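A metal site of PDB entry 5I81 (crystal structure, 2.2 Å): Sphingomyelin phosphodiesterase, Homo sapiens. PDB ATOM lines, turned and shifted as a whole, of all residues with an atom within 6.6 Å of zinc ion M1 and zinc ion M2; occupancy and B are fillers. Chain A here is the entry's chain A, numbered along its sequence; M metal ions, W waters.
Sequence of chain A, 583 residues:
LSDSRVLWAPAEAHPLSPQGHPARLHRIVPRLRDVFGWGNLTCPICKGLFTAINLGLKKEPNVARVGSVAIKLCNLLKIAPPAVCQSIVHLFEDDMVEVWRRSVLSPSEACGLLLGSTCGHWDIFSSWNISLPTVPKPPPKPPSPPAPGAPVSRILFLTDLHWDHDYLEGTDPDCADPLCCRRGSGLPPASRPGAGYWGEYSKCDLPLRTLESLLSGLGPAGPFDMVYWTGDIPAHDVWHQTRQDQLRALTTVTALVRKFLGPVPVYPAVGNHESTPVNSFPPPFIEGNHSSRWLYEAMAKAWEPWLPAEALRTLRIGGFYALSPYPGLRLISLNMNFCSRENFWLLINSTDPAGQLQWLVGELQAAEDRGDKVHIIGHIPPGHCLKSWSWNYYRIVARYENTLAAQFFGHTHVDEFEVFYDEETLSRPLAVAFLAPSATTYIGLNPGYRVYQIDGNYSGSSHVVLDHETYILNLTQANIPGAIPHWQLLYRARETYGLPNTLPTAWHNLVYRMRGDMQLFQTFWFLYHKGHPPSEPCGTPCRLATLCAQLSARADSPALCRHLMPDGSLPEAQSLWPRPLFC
A ring nitrogen (ND1) of His 413 lies within hydrogen-bond range of the backbone carbonyl oxygen (O) of Tyr 442, at 2.7 Å.
The backbone NH of His 273 lies within hydrogen-bond range of the side-chain carboxylate of Asp 232, at 3.0 Å.
N of Ser 438 lies within hydrogen-bond range of O of His 413.
The backbone NH of His 162 is in hydrogen-bond range of the backbone carbonyl oxygen of Asp 232, 3.0 Å away.
O of His 379 is in hydrogen-bond range of N of Gly 410 (2.9 Å).
N of Thr 440 sits at hydrogen-bond distance from O of Asp 160, at 3.1 Å.
O of Gly 231 lies within hydrogen-bond range of N of Asp 160.
The backbone NH (N) of His 411 lies within hydrogen-bond range of the side-chain carboxylate (OD2) of Asp 160 (3.0 Å).
Five residues have an atom within 4 Å of zinc ion M1: Asp 160, Asp 232, Asn 272, His 379 and His 411.
His 162 touches zinc ion M2.
Four residues have an atom within 4 Å of zinc ion M2: Asp 160, His 162, Asp 232 and His 413.
Zinc ion M2 is bound by a ring nitrogen (NE2) of His 413 (2.0 Å), the side-chain carboxylate of Asp 160 (2.2 Å), the side-chain carboxylate of Asp 232 (2.2 Å) and water W1 (2.4 Å).
Zinc ion M2 has four donor atoms within binding distance.
Zinc ion M1 is bound by water W1 (1.9 Å), NE2 of His 379 (2.1 Å), OD1 of Asn 272 (2.2 Å), ND1 of His 411 (2.2 Å) and OD2 of Asp 232 (2.4 Å).
Zinc ion M1 has five donor atoms within binding distance.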
ATOM      1  N   THR A 159     -31.395   3.777  14.386  1.00  0.00           N
ATOM      2  CA  THR A 159     -30.410   4.212  13.406  1.00  0.00           C
ATOM      3  C   THR A 159     -30.835   5.534  12.778  1.00  0.00           C
ATOM      4  O   THR A 159     -32.032   5.858  12.695  1.00  0.00           O
ATOM      5  CB  THR A 159     -30.183   3.125  12.346  1.00  0.00           C
ATOM      6  OG1 THR A 159     -29.043   3.456  11.555  1.00  0.00           O
ATOM      7  CG2 THR A 159     -31.407   2.950  11.455  1.00  0.00           C
ATOM      8  N   ASP A 160     -29.845   6.331  12.369  1.00  0.00           N
ATOM      9  CA  ASP A 160     -30.099   7.589  11.676  1.00  0.00           C
ATOM     10  C   ASP A 160     -31.078   8.470  12.454  1.00  0.00           C
ATOM     11  O   ASP A 160     -32.158   8.845  11.980  1.00  0.00           O
ATOM     12  CB  ASP A 160     -30.571   7.331  10.240  1.00  0.00           C
ATOM     13  CG  ASP A 160     -29.593   6.440   9.480  1.00  0.00           C
ATOM     14  OD1 ASP A 160     -28.627   7.027   8.917  1.00  0.00           O
ATOM     15  OD2 ASP A 160     -29.723   5.198   9.478  1.00  0.00           O
ATOM     16  N   LEU A 161     -30.657   8.801  13.677  1.00  0.00           N
ATOM     17  CA  LEU A 161     -31.486   9.650  14.523  1.00  0.00           C
ATOM     18  C   LEU A 161     -31.454  11.108  14.034  1.00  0.00           C
ATOM     19  O   LEU A 161     -32.469  11.795  14.082  1.00  0.00           O
ATOM     20  CB  LEU A 161     -31.049   9.525  15.984  1.00  0.00           C
ATOM     21  CG  LEU A 161     -31.642   8.359  16.810  1.00  0.00           C
ATOM     22  CD1 LEU A 161     -31.491   6.940  16.146  1.00  0.00           C
ATOM     23  CD2 LEU A 161     -30.983   8.390  18.173  1.00  0.00           C
ATOM     24  N   HIS A 162     -30.302  11.577  13.551  1.00  0.00           N
ATOM     25  CA  HIS A 162     -30.166  12.907  12.925  1.00  0.00           C
ATOM     26  C   HIS A 162     -30.852  14.029  13.723  1.00  0.00           C
ATOM     27  O   HIS A 162     -31.755  14.730  13.233  1.00  0.00           O
ATOM     28  CB  HIS A 162     -30.704  12.886  11.493  1.00  0.00           C
ATOM     29  CG  HIS A 162     -29.775  12.218  10.535  1.00  0.00           C
ATOM     30  ND1 HIS A 162     -30.073  11.017   9.930  1.00  0.00           N
ATOM     31  CD2 HIS A 162     -28.538  12.570  10.104  1.00  0.00           C
ATOM     32  CE1 HIS A 162     -29.075  10.681   9.137  1.00  0.00           C
ATOM     33  NE2 HIS A 162     -28.122  11.595   9.240  1.00  0.00           N
ATOM     34  N   GLY A 231     -25.605   4.584  14.032  1.00  0.00           N
ATOM     35  CA  GLY A 231     -24.919   5.737  13.478  1.00  0.00           C
ATOM     36  C   GLY A 231     -25.844   6.805  12.905  1.00  0.00           C
ATOM     37  O   GLY A 231     -27.034   6.589  12.658  1.00  0.00           O
ATOM     38  N   ASP A 232     -25.222   7.980  12.706  1.00  0.00           N
ATOM     39  CA  ASP A 232     -25.782   9.238  12.185  1.00  0.00           C
ATOM     40  C   ASP A 232     -26.530   9.989  13.288  1.00  0.00           C
ATOM     41  O   ASP A 232     -27.758   9.944  13.353  1.00  0.00           O
ATOM     42  CB  ASP A 232     -26.688   9.006  10.998  1.00  0.00           C
ATOM     43  CG  ASP A 232     -25.947   9.040   9.658  1.00  0.00           C
ATOM     44  OD1 ASP A 232     -24.692   9.037   9.590  1.00  0.00           O
ATOM     45  OD2 ASP A 232     -26.684   9.055   8.639  1.00  0.00           O
ATOM     46  N   HIS A 236     -28.456  17.006   8.821  1.00  0.00           N
ATOM     47  CA  HIS A 236     -27.911  17.239   7.482  1.00  0.00           C
ATOM     48  C   HIS A 236     -27.548  18.704   7.239  1.00  0.00           C
ATOM     49  O   HIS A 236     -27.447  19.120   6.077  1.00  0.00           O
ATOM     50  CB  HIS A 236     -28.891  16.749   6.411  1.00  0.00           C
ATOM     51  CG  HIS A 236     -29.181  15.268   6.475  1.00  0.00           C
ATOM     52  ND1 HIS A 236     -30.017  14.718   7.431  1.00  0.00           N
ATOM     53  CD2 HIS A 236     -28.715  14.228   5.727  1.00  0.00           C
ATOM     54  CE1 HIS A 236     -30.050  13.403   7.265  1.00  0.00           C
ATOM     55  NE2 HIS A 236     -29.277  13.079   6.242  1.00  0.00           N
ATOM     56  N   GLY A 271     -21.615   6.388  12.022  1.00  0.00           N
ATOM     57  CA  GLY A 271     -22.278   6.800  10.793  1.00  0.00           C
ATOM     58  C   GLY A 271     -21.406   7.742   9.990  1.00  0.00           C
ATOM     59  O   GLY A 271     -20.351   8.176  10.458  1.00  0.00           O
ATOM     60  N   ASN A 272     -21.856   8.059   8.762  1.00  0.00           N
ATOM     61  CA  ASN A 272     -21.088   8.968   7.925  1.00  0.00           C
ATOM     62  C   ASN A 272     -21.267  10.428   8.324  1.00  0.00           C
ATOM     63  O   ASN A 272     -20.495  11.272   7.853  1.00  0.00           O
ATOM     64  CB  ASN A 272     -21.467   8.782   6.441  1.00  0.00           C
ATOM     65  CG  ASN A 272     -22.937   9.019   6.184  1.00  0.00           C
ATOM     66  OD1 ASN A 272     -23.806   8.424   6.837  1.00  0.00           O
ATOM     67  ND2 ASN A 272     -23.239   9.927   5.236  1.00  0.00           N
ATOM     68  N   HIS A 273     -22.221  10.760   9.196  1.00  0.00           N
ATOM     69  CA  HIS A 273     -22.452  12.144   9.574  1.00  0.00           C
ATOM     70  C   HIS A 273     -21.794  12.530  10.883  1.00  0.00           C
ATOM     71  O   HIS A 273     -21.882  13.705  11.275  1.00  0.00           O
ATOM     72  CB  HIS A 273     -23.945  12.470   9.653  1.00  0.00           C
ATOM     73  CG  HIS A 273     -24.563  12.752   8.318  1.00  0.00           C
ATOM     74  ND1 HIS A 273     -24.783  14.028   7.867  1.00  0.00           N
ATOM     75  CD2 HIS A 273     -25.019  11.913   7.336  1.00  0.00           C
ATOM     76  CE1 HIS A 273     -25.318  13.976   6.658  1.00  0.00           C
ATOM     77  NE2 HIS A 273     -25.466  12.718   6.313  1.00  0.00           N
ATOM     78  N   ASN A 279     -18.823  12.790   5.947  1.00  0.00           N
ATOM     79  CA  ASN A 279     -18.102  11.734   5.222  1.00  0.00           C
ATOM     80  C   ASN A 279     -16.578  11.799   5.342  1.00  0.00           C
ATOM     81  O   ASN A 279     -15.879  10.972   4.709  1.00  0.00           O
ATOM     82  CB  ASN A 279     -18.449  11.708   3.714  1.00  0.00           C
ATOM     83  CG  ASN A 279     -19.964  11.610   3.451  1.00  0.00           C
ATOM     84  OD1 ASN A 279     -20.522  12.451   2.731  1.00  0.00           O
ATOM     85  ND2 ASN A 279     -20.626  10.610   4.023  1.00  0.00           N
ATOM     86  N   HIS A 379     -23.162   0.968   9.436  1.00  0.00           N
ATOM     87  CA  HIS A 379     -24.018   2.032   8.967  1.00  0.00           C
ATOM     88  C   HIS A 379     -24.325   1.901   7.482  1.00  0.00           C
ATOM     89  O   HIS A 379     -25.419   1.464   7.114  1.00  0.00           O
ATOM     90  CB  HIS A 379     -23.370   3.387   9.271  1.00  0.00           C
ATOM     91  CG  HIS A 379     -24.247   4.540   8.943  1.00  0.00           C
ATOM     92  ND1 HIS A 379     -25.404   4.808   9.634  1.00  0.00           N
ATOM     93  CD2 HIS A 379     -24.165   5.462   7.949  1.00  0.00           C
ATOM     94  CE1 HIS A 379     -25.998   5.861   9.088  1.00  0.00           C
ATOM     95  NE2 HIS A 379     -25.252   6.273   8.075  1.00  0.00           N
ATOM     96  N   ILE A 380     -23.387   2.302   6.619  1.00  0.00           N
ATOM     97  CA  ILE A 380     -23.592   2.172   5.161  1.00  0.00           C
ATOM     98  C   ILE A 380     -23.734   0.693   4.808  1.00  0.00           C
ATOM     99  O   ILE A 380     -22.832  -0.099   5.156  1.00  0.00           O
ATOM    100  CB  ILE A 380     -22.416   2.803   4.402  1.00  0.00           C
ATOM    101  CG1 ILE A 380     -22.260   4.291   4.750  1.00  0.00           C
ATOM    102  CG2 ILE A 380     -22.515   2.531   2.915  1.00  0.00           C
ATOM    103  CD1 ILE A 380     -20.987   4.942   4.224  1.00  0.00           C
ATOM    104  N   GLY A 410     -27.872   0.483   8.246  1.00  0.00           N
ATOM    105  CA  GLY A 410     -28.807   1.592   8.190  1.00  0.00           C
ATOM    106  C   GLY A 410     -28.534   2.457   6.976  1.00  0.00           C
ATOM    107  O   GLY A 410     -28.442   1.958   5.839  1.00  0.00           O
ATOM    108  N   HIS A 411     -28.426   3.766   7.222  1.00  0.00           N
ATOM    109  CA  HIS A 411     -27.932   4.748   6.255  1.00  0.00           C
ATOM    110  C   HIS A 411     -28.927   5.107   5.143  1.00  0.00           C
ATOM    111  O   HIS A 411     -29.026   6.297   4.832  1.00  0.00           O
ATOM    112  CB  HIS A 411     -26.621   4.291   5.602  1.00  0.00           C
ATOM    113  CG  HIS A 411     -26.057   5.268   4.611  1.00  0.00           C
ATOM    114  ND1 HIS A 411     -25.618   6.526   4.967  1.00  0.00           N
ATOM    115  CD2 HIS A 411     -25.809   5.147   3.279  1.00  0.00           C
ATOM    116  CE1 HIS A 411     -25.150   7.145   3.899  1.00  0.00           C
ATOM    117  NE2 HIS A 411     -25.253   6.328   2.863  1.00  0.00           N
ATOM    118  N   THR A 412     -29.674   4.147   4.553  1.00  0.00           N
ATOM    119  CA  THR A 412     -30.585   4.555   3.461  1.00  0.00           C
ATOM    120  C   THR A 412     -31.885   5.165   3.971  1.00  0.00           C
ATOM    121  O   THR A 412     -32.612   5.768   3.191  1.00  0.00           O
ATOM    122  CB  THR A 412     -30.950   3.373   2.531  1.00  0.00           C
ATOM    123  OG1 THR A 412     -31.782   2.435   3.234  1.00  0.00           O
ATOM    124  CG2 THR A 412     -29.711   2.637   2.052  1.00  0.00           C
ATOM    125  N   HIS A 413     -32.213   4.998   5.241  1.00  0.00           N
ATOM    126  CA  HIS A 413     -33.380   5.584   5.903  1.00  0.00           C
ATOM    127  C   HIS A 413     -34.692   4.893   5.544  1.00  0.00           C
ATOM    128  O   HIS A 413     -35.698   5.189   6.176  1.00  0.00           O
ATOM    129  CB  HIS A 413     -33.558   7.102   5.646  1.00  0.00           C
ATOM    130  CG  HIS A 413     -32.465   7.961   6.205  1.00  0.00           C
ATOM    131  ND1 HIS A 413     -32.568   9.333   6.271  1.00  0.00           N
ATOM    132  CD2 HIS A 413     -31.267   7.647   6.741  1.00  0.00           C
ATOM    133  CE1 HIS A 413     -31.449   9.837   6.781  1.00  0.00           C
ATOM    134  NE2 HIS A 413     -30.651   8.832   7.086  1.00  0.00           N
ATOM    135  N   SER A 438     -35.098   4.873   9.212  1.00  0.00           N
ATOM    136  CA  SER A 438     -34.473   5.878  10.076  1.00  0.00           C
ATOM    137  C   SER A 438     -35.433   6.416  11.132  1.00  0.00           C
ATOM    138  O   SER A 438     -36.658   6.468  10.941  1.00  0.00           O
ATOM    139  CB  SER A 438     -33.943   7.053   9.241  1.00  0.00           C
ATOM    140  OG  SER A 438     -35.008   7.672   8.525  1.00  0.00           O
ATOM    141  N   THR A 440     -35.150   9.504  11.808  1.00  0.00           N
ATOM    142  CA  THR A 440     -35.446  10.825  11.253  1.00  0.00           C
ATOM    143  C   THR A 440     -36.505  10.754  10.162  1.00  0.00           C
ATOM    144  O   THR A 440     -36.708   9.724   9.508  1.00  0.00           O
ATOM    145  CB  THR A 440     -34.208  11.501  10.648  1.00  0.00           C
ATOM    146  OG1 THR A 440     -34.571  12.827  10.265  1.00  0.00           O
ATOM    147  CG2 THR A 440     -33.688  10.733   9.366  1.00  0.00           C
ATOM    148  N   TYR A 442     -36.105  12.639   7.472  1.00  0.00           N
ATOM    149  CA  TYR A 442     -35.388  12.978   6.245  1.00  0.00           C
ATOM    150  C   TYR A 442     -35.324  11.819   5.264  1.00  0.00           C
ATOM    151  O   TYR A 442     -34.702  10.791   5.595  1.00  0.00           O
ATOM    152  CB  TYR A 442     -33.946  13.394   6.615  1.00  0.00           C
ATOM    153  CG  TYR A 442     -33.123  14.016   5.482  1.00  0.00           C
ATOM    154  CD1 TYR A 442     -33.104  15.404   5.274  1.00  0.00           C
ATOM    155  CD2 TYR A 442     -32.317  13.218   4.652  1.00  0.00           C
ATOM    156  CE1 TYR A 442     -32.335  15.980   4.239  1.00  0.00           C
ATOM    157  CE2 TYR A 442     -31.542  13.783   3.611  1.00  0.00           C
ATOM    158  CZ  TYR A 442     -31.568  15.153   3.426  1.00  0.00           C
ATOM    159  OH  TYR A 442     -30.814  15.700   2.432  1.00  0.00           O
HETATM  160 ZN    ZN M   1     -25.864   7.797   6.772  1.00  0.00          ZN
HETATM  161 ZN    ZN M   2     -28.767   8.948   7.867  1.00  0.00          ZN
HETATM  162  O   HOH W   1     -27.395   8.553   5.989  1.00  0.00           O
